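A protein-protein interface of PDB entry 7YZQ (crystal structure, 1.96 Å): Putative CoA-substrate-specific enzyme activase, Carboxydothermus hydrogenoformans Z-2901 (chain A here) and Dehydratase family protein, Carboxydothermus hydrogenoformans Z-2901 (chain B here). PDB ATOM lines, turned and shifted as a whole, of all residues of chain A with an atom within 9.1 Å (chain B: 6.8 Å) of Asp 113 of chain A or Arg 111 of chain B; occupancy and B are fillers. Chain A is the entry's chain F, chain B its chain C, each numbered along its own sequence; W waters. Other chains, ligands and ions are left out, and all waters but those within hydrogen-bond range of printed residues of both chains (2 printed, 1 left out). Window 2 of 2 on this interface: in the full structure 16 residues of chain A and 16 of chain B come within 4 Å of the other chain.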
ATOM      1  N   GLN A  93       9.371  15.062 -12.761  1.00  0.00           N
ATOM      2  CA  GLN A  93      10.467  15.623 -13.547  1.00  0.00           C
ATOM      3  C   GLN A  93      11.143  14.633 -14.503  1.00  0.00           C
ATOM      4  O   GLN A  93      11.609  15.049 -15.593  1.00  0.00           O
ATOM      5  CB  GLN A  93      11.489  16.249 -12.574  1.00  0.00           C
ATOM      6  CG  GLN A  93      12.902  16.436 -13.091  1.00  0.00           C
ATOM      7  CD  GLN A  93      13.089  17.702 -13.949  1.00  0.00           C
ATOM      8  OE1 GLN A  93      14.103  17.837 -14.651  1.00  0.00           O
ATOM      9  NE2 GLN A  93      12.120  18.623 -13.885  1.00  0.00           N
ATOM     10  N   ASP A  94      11.226  13.353 -14.137  1.00  0.00           N
ATOM     11  CA  ASP A  94      11.929  12.342 -14.921  1.00  0.00           C
ATOM     12  C   ASP A  94      10.979  11.280 -15.437  1.00  0.00           C
ATOM     13  O   ASP A  94       9.958  10.973 -14.810  1.00  0.00           O
ATOM     14  CB  ASP A  94      13.048  11.640 -14.091  1.00  0.00           C
ATOM     15  CG  ASP A  94      14.079  12.609 -13.611  1.00  0.00           C
ATOM     16  OD1 ASP A  94      14.986  12.960 -14.415  1.00  0.00           O
ATOM     17  OD2 ASP A  94      13.961  13.042 -12.434  1.00  0.00           O
ATOM     18  N   ALA A  95      11.332  10.756 -16.613  1.00  0.00           N
ATOM     19  CA  ALA A  95      10.728   9.572 -17.202  1.00  0.00           C
ATOM     20  C   ALA A  95      11.774   8.467 -17.295  1.00  0.00           C
ATOM     21  O   ALA A  95      12.935   8.727 -17.633  1.00  0.00           O
ATOM     22  CB  ALA A  95      10.163   9.887 -18.593  1.00  0.00           C
ATOM     23  N   LYS A  96      11.365   7.231 -17.002  1.00  0.00           N
ATOM     24  CA  LYS A  96      12.314   6.128 -16.884  1.00  0.00           C
ATOM     25  C   LYS A  96      11.753   4.842 -17.498  1.00  0.00           C
ATOM     26  O   LYS A  96      10.599   4.464 -17.273  1.00  0.00           O
ATOM     27  CB  LYS A  96      12.728   5.839 -15.404  1.00  0.00           C
ATOM     28  CG  LYS A  96      12.976   7.057 -14.490  1.00  0.00           C
ATOM     29  CD  LYS A  96      11.647   7.533 -13.882  1.00  0.00           C
ATOM     30  CE  LYS A  96      11.867   8.544 -12.768  1.00  0.00           C
ATOM     31  NZ  LYS A  96      10.510   9.139 -12.358  1.00  0.00           N
ATOM     32  N   LEU A 110      16.942   3.481 -19.040  1.00  0.00           N
ATOM     33  CA  LEU A 110      17.126   4.728 -19.770  1.00  0.00           C
ATOM     34  C   LEU A 110      16.229   5.782 -19.141  1.00  0.00           C
ATOM     35  O   LEU A 110      15.054   5.528 -18.889  1.00  0.00           O
ATOM     36  CB  LEU A 110      16.787   4.543 -21.259  1.00  0.00           C
ATOM     37  CG  LEU A 110      16.719   5.807 -22.122  1.00  0.00           C
ATOM     38  CD1 LEU A 110      18.010   6.606 -21.926  1.00  0.00           C
ATOM     39  CD2 LEU A 110      16.495   5.440 -23.574  1.00  0.00           C
ATOM     40  N   MET A 111      16.780   6.958 -18.898  1.00  0.00           N
ATOM     41  CA  MET A 111      16.019   8.086 -18.388  1.00  0.00           C
ATOM     42  C   MET A 111      15.974   9.173 -19.453  1.00  0.00           C
ATOM     43  O   MET A 111      16.742   9.172 -20.414  1.00  0.00           O
ATOM     44  CB  MET A 111      16.622   8.616 -17.083  1.00  0.00           C
ATOM     45  CG  MET A 111      16.603   7.568 -15.972  1.00  0.00           C
ATOM     46  SD  MET A 111      17.157   8.167 -14.388  1.00  0.00           S
ATOM     47  CE  MET A 111      15.949   9.462 -14.026  1.00  0.00           C
ATOM     48  N   ASN A 112      15.021  10.081 -19.288  1.00  0.00           N
ATOM     49  CA  ASN A 112      14.745  11.083 -20.303  1.00  0.00           C
ATOM     50  C   ASN A 112      15.959  11.967 -20.529  1.00  0.00           C
ATOM     51  O   ASN A 112      16.763  12.179 -19.619  1.00  0.00           O
ATOM     52  CB  ASN A 112      13.560  11.937 -19.870  1.00  0.00           C
ATOM     53  CG  ASN A 112      13.792  12.639 -18.530  1.00  0.00           C
ATOM     54  OD1 ASN A 112      13.659  12.024 -17.468  1.00  0.00           O
ATOM     55  ND2 ASN A 112      14.148  13.931 -18.575  1.00  0.00           N
ATOM     56  N   ASP A 113      16.077  12.509 -21.749  1.00  0.00           N
ATOM     57  CA  ASP A 113      17.093  13.520 -22.024  1.00  0.00           C
ATOM     58  C   ASP A 113      16.696  14.876 -21.404  1.00  0.00           C
ATOM     59  O   ASP A 113      15.600  15.053 -20.863  1.00  0.00           O
ATOM     60  CB  ASP A 113      17.312  13.657 -23.529  1.00  0.00           C
ATOM     61  CG  ASP A 113      16.025  13.994 -24.262  1.00  0.00           C
ATOM     62  OD1 ASP A 113      15.319  14.961 -23.847  1.00  0.00           O
ATOM     63  OD2 ASP A 113      15.713  13.324 -25.271  1.00  0.00           O
ATOM     64  N   LYS A 114      17.580  15.864 -21.522  1.00  0.00           N
ATOM     65  CA  LYS A 114      17.336  17.138 -20.844  1.00  0.00           C
ATOM     66  C   LYS A 114      16.103  17.845 -21.394  1.00  0.00           C
ATOM     67  O   LYS A 114      15.313  18.420 -20.622  1.00  0.00           O
ATOM     68  CB  LYS A 114      18.568  18.037 -20.954  1.00  0.00           C
ATOM     69  CG  LYS A 114      19.673  17.716 -19.914  1.00  0.00           C
ATOM     70  CD  LYS A 114      20.910  18.575 -20.077  1.00  0.00           C
ATOM     71  CE  LYS A 114      20.761  19.917 -19.380  1.00  0.00           C
ATOM     72  NZ  LYS A 114      20.111  19.868 -18.029  1.00  0.00           N
ATOM     73  N   CYS A 115      15.896  17.796 -22.718  1.00  0.00           N
ATOM     74  CA  CYS A 115      14.755  18.499 -23.285  1.00  0.00           C
ATOM     75  C   CYS A 115      13.425  17.817 -22.996  1.00  0.00           C
ATOM     76  O   CYS A 115      12.360  18.428 -23.235  1.00  0.00           O
ATOM     77  CB  CYS A 115      14.892  18.652 -24.783  1.00  0.00           C
ATOM     78  SG  CYS A 115      16.278  19.603 -25.288  1.00  0.00           S
ATOM     79  N   ALA A 116      13.467  16.574 -22.501  1.00  0.00           N
ATOM     80  CA  ALA A 116      12.276  15.834 -22.124  1.00  0.00           C
ATOM     81  C   ALA A 116      11.986  15.911 -20.633  1.00  0.00           C
ATOM     82  O   ALA A 116      11.101  15.187 -20.151  1.00  0.00           O
ATOM     83  CB  ALA A 116      12.400  14.376 -22.546  1.00  0.00           C
ATOM     84  N   ALA A 117      12.680  16.784 -19.908  1.00  0.00           N
ATOM     85  CA  ALA A 117      12.470  16.903 -18.478  1.00  0.00           C
ATOM     86  C   ALA A 117      11.154  17.601 -18.168  1.00  0.00           C
ATOM     87  O   ALA A 117      10.661  18.434 -18.935  1.00  0.00           O
ATOM     88  CB  ALA A 117      13.602  17.664 -17.838  1.00  0.00           C
ATOM     89  N   GLY A 118      10.550  17.209 -17.047  1.00  0.00           N
ATOM     90  CA  GLY A 118       9.405  17.944 -16.539  1.00  0.00           C
ATOM     91  C   GLY A 118       8.085  17.653 -17.197  1.00  0.00           C
ATOM     92  O   GLY A 118       7.152  18.444 -17.043  1.00  0.00           O
ATOM     93  N   THR A 119       7.968  16.537 -17.922  1.00  0.00           N
ATOM     94  CA  THR A 119       6.711  16.214 -18.601  1.00  0.00           C
ATOM     95  C   THR A 119       5.555  16.110 -17.602  1.00  0.00           C
ATOM     96  O   THR A 119       4.478  16.704 -17.802  1.00  0.00           O
ATOM     97  CB  THR A 119       6.864  14.907 -19.397  1.00  0.00           C
ATOM     98  OG1 THR A 119       8.038  14.988 -20.226  1.00  0.00           O
ATOM     99  CG2 THR A 119       5.629  14.622 -20.251  1.00  0.00           C
ATOM    100  N   ASN A 149       3.202  19.751 -29.977  1.00  0.00           N
ATOM    101  CA  ASN A 149       4.622  19.485 -30.185  1.00  0.00           C
ATOM    102  C   ASN A 149       5.151  18.586 -29.082  1.00  0.00           C
ATOM    103  O   ASN A 149       4.833  18.767 -27.905  1.00  0.00           O
ATOM    104  CB  ASN A 149       5.408  20.806 -30.219  1.00  0.00           C
ATOM    105  CG  ASN A 149       6.717  20.695 -30.952  1.00  0.00           C
ATOM    106  OD1 ASN A 149       7.423  19.702 -30.830  1.00  0.00           O
ATOM    107  ND2 ASN A 149       7.056  21.729 -31.726  1.00  0.00           N
ATOM    108  N   SER A 150       5.958  17.605 -29.468  1.00  0.00           N
ATOM    109  CA  SER A 150       6.515  16.639 -28.529  1.00  0.00           C
ATOM    110  C   SER A 150       7.952  16.968 -28.149  1.00  0.00           C
ATOM    111  O   SER A 150       8.549  16.246 -27.350  1.00  0.00           O
ATOM    112  CB  SER A 150       6.443  15.216 -29.130  1.00  0.00           C
ATOM    113  OG  SER A 150       6.996  15.153 -30.454  1.00  0.00           O
ATOM    114  N   MET A 151       8.516  18.049 -28.686  1.00  0.00           N
ATOM    115  CA  MET A 151       9.894  18.400 -28.375  1.00  0.00           C
ATOM    116  C   MET A 151      10.130  18.535 -26.871  1.00  0.00           C
ATOM    117  O   MET A 151      11.071  17.944 -26.329  1.00  0.00           O
ATOM    118  CB  MET A 151      10.266  19.701 -29.083  1.00  0.00           C
ATOM    119  CG  MET A 151      11.661  20.143 -28.857  1.00  0.00           C
ATOM    120  SD  MET A 151      12.811  19.029 -29.752  1.00  0.00           S
ATOM    121  CE  MET A 151      12.755  19.615 -31.406  1.00  0.00           C
ATOM    122  N   CYS A 152       9.350  19.379 -26.201  1.00  0.00           N
ATOM    123  CA  CYS A 152       9.592  19.728 -24.810  1.00  0.00           C
ATOM    124  C   CYS A 152       8.372  20.483 -24.336  1.00  0.00           C
ATOM    125  O   CYS A 152       7.494  20.849 -25.128  1.00  0.00           O
ATOM    126  CB  CYS A 152      10.859  20.571 -24.675  1.00  0.00           C
ATOM    127  SG  CYS A 152      10.644  22.162 -25.540  1.00  0.00           S
ATOM    128  N   THR A 153       8.347  20.747 -23.036  1.00  0.00           N
ATOM    129  CA  THR A 153       7.207  21.428 -22.445  1.00  0.00           C
ATOM    130  C   THR A 153       7.193  22.930 -22.751  1.00  0.00           C
ATOM    131  O   THR A 153       6.121  23.537 -22.675  1.00  0.00           O
ATOM    132  CB  THR A 153       7.146  21.240 -20.913  1.00  0.00           C
ATOM    133  OG1 THR A 153       8.289  21.835 -20.326  1.00  0.00           O
ATOM    134  CG2 THR A 153       7.071  19.794 -20.538  1.00  0.00           C
ATOM    135  N   PHE A 155       7.930  24.271 -25.851  1.00  0.00           N
ATOM    136  CA  PHE A 155       7.247  24.353 -27.144  1.00  0.00           C
ATOM    137  C   PHE A 155       5.777  23.940 -27.016  1.00  0.00           C
ATOM    138  O   PHE A 155       4.915  24.440 -27.747  1.00  0.00           O
ATOM    139  CB  PHE A 155       7.930  23.451 -28.179  1.00  0.00           C
ATOM    140  CG  PHE A 155       9.304  23.889 -28.625  1.00  0.00           C
ATOM    141  CD1 PHE A 155      10.071  24.720 -27.870  1.00  0.00           C
ATOM    142  CD2 PHE A 155       9.816  23.429 -29.838  1.00  0.00           C
ATOM    143  CE1 PHE A 155      11.357  25.106 -28.282  1.00  0.00           C
ATOM    144  CE2 PHE A 155      11.066  23.784 -30.274  1.00  0.00           C
ATOM    145  CZ  PHE A 155      11.861  24.636 -29.485  1.00  0.00           C
ATOM    146  N   THR A 180      -0.309  13.064 -27.460  1.00  0.00           N
ATOM    147  CA  THR A 180       1.084  13.310 -27.823  1.00  0.00           C
ATOM    148  C   THR A 180       2.025  12.786 -26.746  1.00  0.00           C
ATOM    149  O   THR A 180       3.114  12.284 -27.047  1.00  0.00           O
ATOM    150  CB  THR A 180       1.311  14.817 -28.057  1.00  0.00           C
ATOM    151  OG1 THR A 180       0.512  15.251 -29.162  1.00  0.00           O
ATOM    152  CG2 THR A 180       2.772  15.137 -28.363  1.00  0.00           C
ATOM    153  N   ARG A 184       4.898   9.814 -27.487  1.00  0.00           N
ATOM    154  CA  ARG A 184       6.332   9.908 -27.211  1.00  0.00           C
ATOM    155  C   ARG A 184       6.777   8.862 -26.174  1.00  0.00           C
ATOM    156  O   ARG A 184       7.848   8.248 -26.290  1.00  0.00           O
ATOM    157  CB  ARG A 184       6.690  11.321 -26.734  1.00  0.00           C
ATOM    158  CG  ARG A 184       8.199  11.609 -26.837  1.00  0.00           C
ATOM    159  CD  ARG A 184       8.624  12.965 -26.236  1.00  0.00           C
ATOM    160  NE  ARG A 184       7.973  13.300 -24.964  1.00  0.00           N
ATOM    161  CZ  ARG A 184       6.826  13.982 -24.873  1.00  0.00           C
ATOM    162  NH1 ARG A 184       6.289  14.269 -23.687  1.00  0.00           N
ATOM    163  NH2 ARG A 184       6.210  14.411 -25.976  1.00  0.00           N
ATOM    164  N   LEU A 185       5.981   8.672 -25.131  1.00  0.00           N
ATOM    165  CA  LEU A 185       6.348   7.730 -24.078  1.00  0.00           C
ATOM    166  C   LEU A 185       6.314   6.288 -24.570  1.00  0.00           C
ATOM    167  O   LEU A 185       7.098   5.456 -24.095  1.00  0.00           O
ATOM    168  CB  LEU A 185       5.401   7.912 -22.884  1.00  0.00           C
ATOM    169  CG  LEU A 185       5.649   9.174 -22.056  1.00  0.00           C
ATOM    170  CD1 LEU A 185       4.511   9.389 -21.094  1.00  0.00           C
ATOM    171  CD2 LEU A 185       6.961   9.096 -21.315  1.00  0.00           C
ATOM    172  N   LYS A 187       7.054   5.288 -27.783  1.00  0.00           N
ATOM    173  CA  LYS A 187       8.355   5.123 -28.424  1.00  0.00           C
ATOM    174  C   LYS A 187       9.479   5.050 -27.390  1.00  0.00           C
ATOM    175  O   LYS A 187      10.403   4.230 -27.517  1.00  0.00           O
ATOM    176  CB  LYS A 187       8.624   6.257 -29.413  1.00  0.00           C
ATOM    177  CG  LYS A 187       7.507   6.512 -30.413  1.00  0.00           C
ATOM    178  CD  LYS A 187       7.409   5.388 -31.447  1.00  0.00           C
ATOM    179  CE  LYS A 187       6.747   5.881 -32.751  1.00  0.00           C
ATOM    180  NZ  LYS A 187       6.178   4.749 -33.568  1.00  0.00           N
ATOM    181  N   PHE A 188       9.422   5.887 -26.358  1.00  0.00           N
ATOM    182  CA  PHE A 188      10.444   5.868 -25.313  1.00  0.00           C
ATOM    183  C   PHE A 188      10.502   4.527 -24.581  1.00  0.00           C
ATOM    184  O   PHE A 188      11.587   4.057 -24.204  1.00  0.00           O
ATOM    185  CB  PHE A 188      10.151   7.019 -24.335  1.00  0.00           C
ATOM    186  CG  PHE A 188      11.091   7.098 -23.168  1.00  0.00           C
ATOM    187  CD1 PHE A 188      12.386   7.512 -23.342  1.00  0.00           C
ATOM    188  CD2 PHE A 188      10.659   6.785 -21.883  1.00  0.00           C
ATOM    189  CE1 PHE A 188      13.236   7.613 -22.263  1.00  0.00           C
ATOM    190  CE2 PHE A 188      11.515   6.871 -20.808  1.00  0.00           C
ATOM    191  CZ  PHE A 188      12.806   7.279 -21.002  1.00  0.00           C
ATOM    192  N   VAL B 102       7.758  12.641 -37.011  1.00  0.00           N
ATOM    193  CA  VAL B 102       8.960  13.044 -36.270  1.00  0.00           C
ATOM    194  C   VAL B 102       9.171  12.110 -35.086  1.00  0.00           C
ATOM    195  O   VAL B 102      10.305  11.698 -34.825  1.00  0.00           O
ATOM    196  CB  VAL B 102       8.868  14.536 -35.869  1.00  0.00           C
ATOM    197  CG1 VAL B 102       9.770  14.894 -34.735  1.00  0.00           C
ATOM    198  CG2 VAL B 102       9.209  15.425 -37.088  1.00  0.00           C
ATOM    199  N   GLU B 106      12.669  10.014 -34.219  1.00  0.00           N
ATOM    200  CA  GLU B 106      13.402  10.138 -32.965  1.00  0.00           C
ATOM    201  C   GLU B 106      13.692   8.791 -32.324  1.00  0.00           C
ATOM    202  O   GLU B 106      14.438   8.735 -31.339  1.00  0.00           O
ATOM    203  CB  GLU B 106      12.618  11.035 -31.993  1.00  0.00           C
ATOM    204  CG  GLU B 106      12.581  12.502 -32.503  1.00  0.00           C
ATOM    205  CD  GLU B 106      11.623  13.403 -31.739  1.00  0.00           C
ATOM    206  OE1 GLU B 106      10.774  12.880 -30.987  1.00  0.00           O
ATOM    207  OE2 GLU B 106      11.743  14.634 -31.913  1.00  0.00           O
ATOM    208  N   LEU B 109      17.200   8.905 -33.985  1.00  0.00           N
ATOM    209  CA  LEU B 109      17.861  10.190 -34.136  1.00  0.00           C
ATOM    210  C   LEU B 109      17.692  11.039 -32.882  1.00  0.00           C
ATOM    211  O   LEU B 109      16.696  10.908 -32.157  1.00  0.00           O
ATOM    212  CB  LEU B 109      17.309  10.981 -35.339  1.00  0.00           C
ATOM    213  CG  LEU B 109      17.587  10.432 -36.761  1.00  0.00           C
ATOM    214  CD1 LEU B 109      16.802  11.212 -37.845  1.00  0.00           C
ATOM    215  CD2 LEU B 109      19.068  10.522 -37.033  1.00  0.00           C
ATOM    216  N   PRO B 110      18.634  11.951 -32.624  1.00  0.00           N
ATOM    217  CA  PRO B 110      18.444  12.925 -31.539  1.00  0.00           C
ATOM    218  C   PRO B 110      17.214  13.783 -31.761  1.00  0.00           C
ATOM    219  O   PRO B 110      16.861  14.107 -32.896  1.00  0.00           O
ATOM    220  CB  PRO B 110      19.718  13.777 -31.590  1.00  0.00           C
ATOM    221  CG  PRO B 110      20.712  12.941 -32.302  1.00  0.00           C
ATOM    222  CD  PRO B 110      19.936  12.132 -33.293  1.00  0.00           C
ATOM    223  N   ARG B 111      16.559  14.177 -30.657  1.00  0.00           N
ATOM    224  CA  ARG B 111      15.395  15.042 -30.812  1.00  0.00           C
ATOM    225  C   ARG B 111      15.807  16.478 -31.136  1.00  0.00           C
ATOM    226  O   ARG B 111      15.056  17.178 -31.831  1.00  0.00           O
ATOM    227  CB  ARG B 111      14.521  14.942 -29.557  1.00  0.00           C
ATOM    228  CG  ARG B 111      14.159  13.474 -29.223  1.00  0.00           C
ATOM    229  CD  ARG B 111      13.084  13.280 -28.156  1.00  0.00           C
ATOM    230  NE  ARG B 111      13.417  14.052 -26.959  1.00  0.00           N
ATOM    231  CZ  ARG B 111      12.680  15.072 -26.547  1.00  0.00           C
ATOM    232  NH1 ARG B 111      13.051  15.770 -25.499  1.00  0.00           N
ATOM    233  NH2 ARG B 111      11.538  15.356 -27.169  1.00  0.00           N
ATOM    234  N   ASN B 112      17.001  16.902 -30.685  1.00  0.00           N
ATOM    235  CA  ASN B 112      17.612  18.182 -31.075  1.00  0.00           C
ATOM    236  C   ASN B 112      18.234  18.100 -32.476  1.00  0.00           C
ATOM    237  O   ASN B 112      19.438  18.245 -32.652  1.00  0.00           O
ATOM    238  CB  ASN B 112      18.739  18.610 -30.137  1.00  0.00           C
ATOM    239  CG  ASN B 112      18.322  18.824 -28.765  1.00  0.00           C
ATOM    240  OD1 ASN B 112      19.114  18.589 -27.828  1.00  0.00           O
ATOM    241  ND2 ASN B 112      17.092  19.255 -28.590  1.00  0.00           N
ATOM    242  N   LEU B 113      17.408  17.850 -33.480  1.00  0.00           N
ATOM    243  CA  LEU B 113      17.897  17.713 -34.849  1.00  0.00           C
ATOM    244  C   LEU B 113      16.867  18.344 -35.754  1.00  0.00           C
ATOM    245  O   LEU B 113      15.705  18.509 -35.361  1.00  0.00           O
ATOM    246  CB  LEU B 113      18.120  16.233 -35.242  1.00  0.00           C
ATOM    247  CG  LEU B 113      19.199  15.942 -36.261  1.00  0.00           C
ATOM    248  CD1 LEU B 113      20.566  16.068 -35.658  1.00  0.00           C
ATOM    249  CD2 LEU B 113      18.979  14.551 -36.909  1.00  0.00           C
ATOM    250  N   CYS B 114      17.316  18.694 -36.961  1.00  0.00           N
ATOM    251  CA  CYS B 114      16.437  19.273 -37.960  1.00  0.00           C
ATOM    252  C   CYS B 114      15.187  18.411 -38.149  1.00  0.00           C
ATOM    253  O   CYS B 114      15.302  17.202 -38.400  1.00  0.00           O
ATOM    254  CB  CYS B 114      17.147  19.427 -39.306  1.00  0.00           C
ATOM    255  SG  CYS B 114      16.241  20.107 -40.632  1.00  0.00           S
ATOM    256  N   PRO B 115      13.994  19.019 -38.147  1.00  0.00           N
ATOM    257  CA  PRO B 115      12.766  18.277 -38.482  1.00  0.00           C
ATOM    258  C   PRO B 115      12.797  17.644 -39.847  1.00  0.00           C
ATOM    259  O   PRO B 115      12.202  16.588 -40.035  1.00  0.00           O
ATOM    260  CB  PRO B 115      11.645  19.341 -38.445  1.00  0.00           C
ATOM    261  CG  PRO B 115      12.293  20.618 -38.026  1.00  0.00           C
ATOM    262  CD  PRO B 115      13.757  20.435 -37.830  1.00  0.00           C
ATOM    263  N   LYS B 118      14.432  14.268 -39.367  1.00  0.00           N
ATOM    264  CA  LYS B 118      13.717  13.373 -38.475  1.00  0.00           C
ATOM    265  C   LYS B 118      12.463  12.846 -39.143  1.00  0.00           C
ATOM    266  O   LYS B 118      12.098  11.680 -38.962  1.00  0.00           O
ATOM    267  CB  LYS B 118      13.373  14.124 -37.175  1.00  0.00           C
ATOM    268  CG  LYS B 118      14.523  14.419 -36.248  1.00  0.00           C
ATOM    269  CD  LYS B 118      14.053  14.905 -34.851  1.00  0.00           C
ATOM    270  CE  LYS B 118      13.442  16.245 -34.906  1.00  0.00           C
ATOM    271  NZ  LYS B 118      12.818  16.657 -33.577  1.00  0.00           N
ATOM    272  N   PHE B 373      17.153  23.821 -35.208  1.00  0.00           N
ATOM    273  CA  PHE B 373      18.367  23.017 -35.128  1.00  0.00           C
ATOM    274  C   PHE B 373      19.063  22.852 -36.474  1.00  0.00           C
ATOM    275  O   PHE B 373      19.946  21.969 -36.594  1.00  0.00           O
ATOM    276  CB  PHE B 373      18.093  21.630 -34.516  1.00  0.00           C
ATOM    277  CG  PHE B 373      17.460  21.706 -33.185  1.00  0.00           C
ATOM    278  CD1 PHE B 373      18.159  22.227 -32.109  1.00  0.00           C
ATOM    279  CD2 PHE B 373      16.168  21.304 -33.000  1.00  0.00           C
ATOM    280  CE1 PHE B 373      17.558  22.351 -30.874  1.00  0.00           C
ATOM    281  CE2 PHE B 373      15.577  21.413 -31.756  1.00  0.00           C
ATOM    282  CZ  PHE B 373      16.270  21.968 -30.713  1.00  0.00           C
HETATM  283  O   HOH W   1      17.096  13.291 -27.900  1.00  0.00           O
HETATM  284  O   HOH W   2      10.491  16.561 -30.808  1.00  0.00           O
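The guanidinium group of Arg 111 of chain B lies close to the backbone NH of Ala 116 of chain A, 3.1 Å away.
The side-chain sulfur of Cys 115 of chain A lies close to the side-chain amide nitrogen of Asn 112 of chain B (3.4 Å).
The backbone carbonyl oxygen of Met 151 of chain A sits at hydrogen-bond distance from the guanidinium group of Arg 111 of chain B, 2.8 Å away.
The backbone carbonyl oxygen (O) of Ser 150 of chain A lies within hydrogen-bond range of the guanidinium group (NH2) of Arg 111 of chain B, 3.1 Å away.
NH1 of Arg 111 of chain B is in salt-bridge range of OD1 of Asp 113 of chain A, 2.9 Å away.
The backbone carbonyl oxygen (O) of Arg 111 of chain B lies within hydrogen-bond range of the side-chain amino group (NZ) of Lys 118 of chain B (2.9 Å).
O of Ala 116 of chain A lies within hydrogen-bond range of OG1 of Thr 119 of chain A, 3.1 Å away.
OE2 of Glu 106 of chain B is in salt-bridge range of NZ of Lys 118 of chain B.
OD1 of Asp 113 of chain A is in hydrogen-bond range of N of Ala 116 of chain A (2.8 Å).
OD1 of Asp 113 of chain A lies within hydrogen-bond range of N of Cys 115 of chain A (3.1 Å).
O of Ser 150 of chain A sits close to NH2 of Arg 184 of chain A (3.3 Å).
Cys 115 of chain A touches Arg 111 of chain B.
CE of Met 151 of chain A touches NZ of Lys 118 of chain B, 3.7 Å away.
Phe 373 of chain B touches Met 151 of chain A (CE2 to CE, 3.4 Å).
NH2 of Arg 111 of chain B touches CD of Arg 184 of chain A, 3.9 Å away.
Of chain B, only Arg 111 comes within 4 Å of Asp 113 of chain A.
Of chain A, only Asp 113 (2.9 Å), Cys 115 (3.3 Å), Ala 116 (3.1 Å), Ser 150 (3.1 Å), Met 151 (2.8 Å) and Arg 184 (3.9 Å) come within 4 Å of Arg 111 of chain B.
No residue of chain A comes within 4 Å of Pro 110 of chain B.
Printed residues of chain B within 4 Å of Cys 115 of chain A: Arg 111 and Asn 112.
Of the printed residues of chain A, Phe 373 of chain B touches Met 151 (3.4 Å).
Leu 113 of chain B touches none of the printed residues of chain A.
Phe 188 of chain A touches none of the printed residues of chain B.
The nearest residue of chain B that does not touch Asp 113 of chain A is Asn 112 of chain B (6.6 Å).
The nearest residue of chain A that does not touch Arg 111 of chain B is Cys 152 of chain A (4.7 Å).
Printed residues of chain B that touch a printed residue of chain A: Arg 111, Asn 112, Lys 118 and Phe 373.
Hydrophobic or aromatic side chains of chain B that line the printed part of chain A: Phe 373.
Of the 25 printed residues of chain A, 6 touch a printed residue of chain B.
Among the printed residues, Asp or Glu carboxylates within 4 Å of a Lys or Arg side-chain nitrogen of the other chain: Asp 113 of chain A with Arg 111 of chain B.
Water W2 lies within hydrogen-bond range of the side-chain carboxylate (OE2) of Glu 106 of chain B (2.5 Å) and the backbone NH (N) of Met 151 of chain A (3.3 Å).
Water W1 lies within hydrogen-bond range of N of Arg 111 of chain B (2.9 Å) and OD2 of Asp 113 of chain A (3.0 Å).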
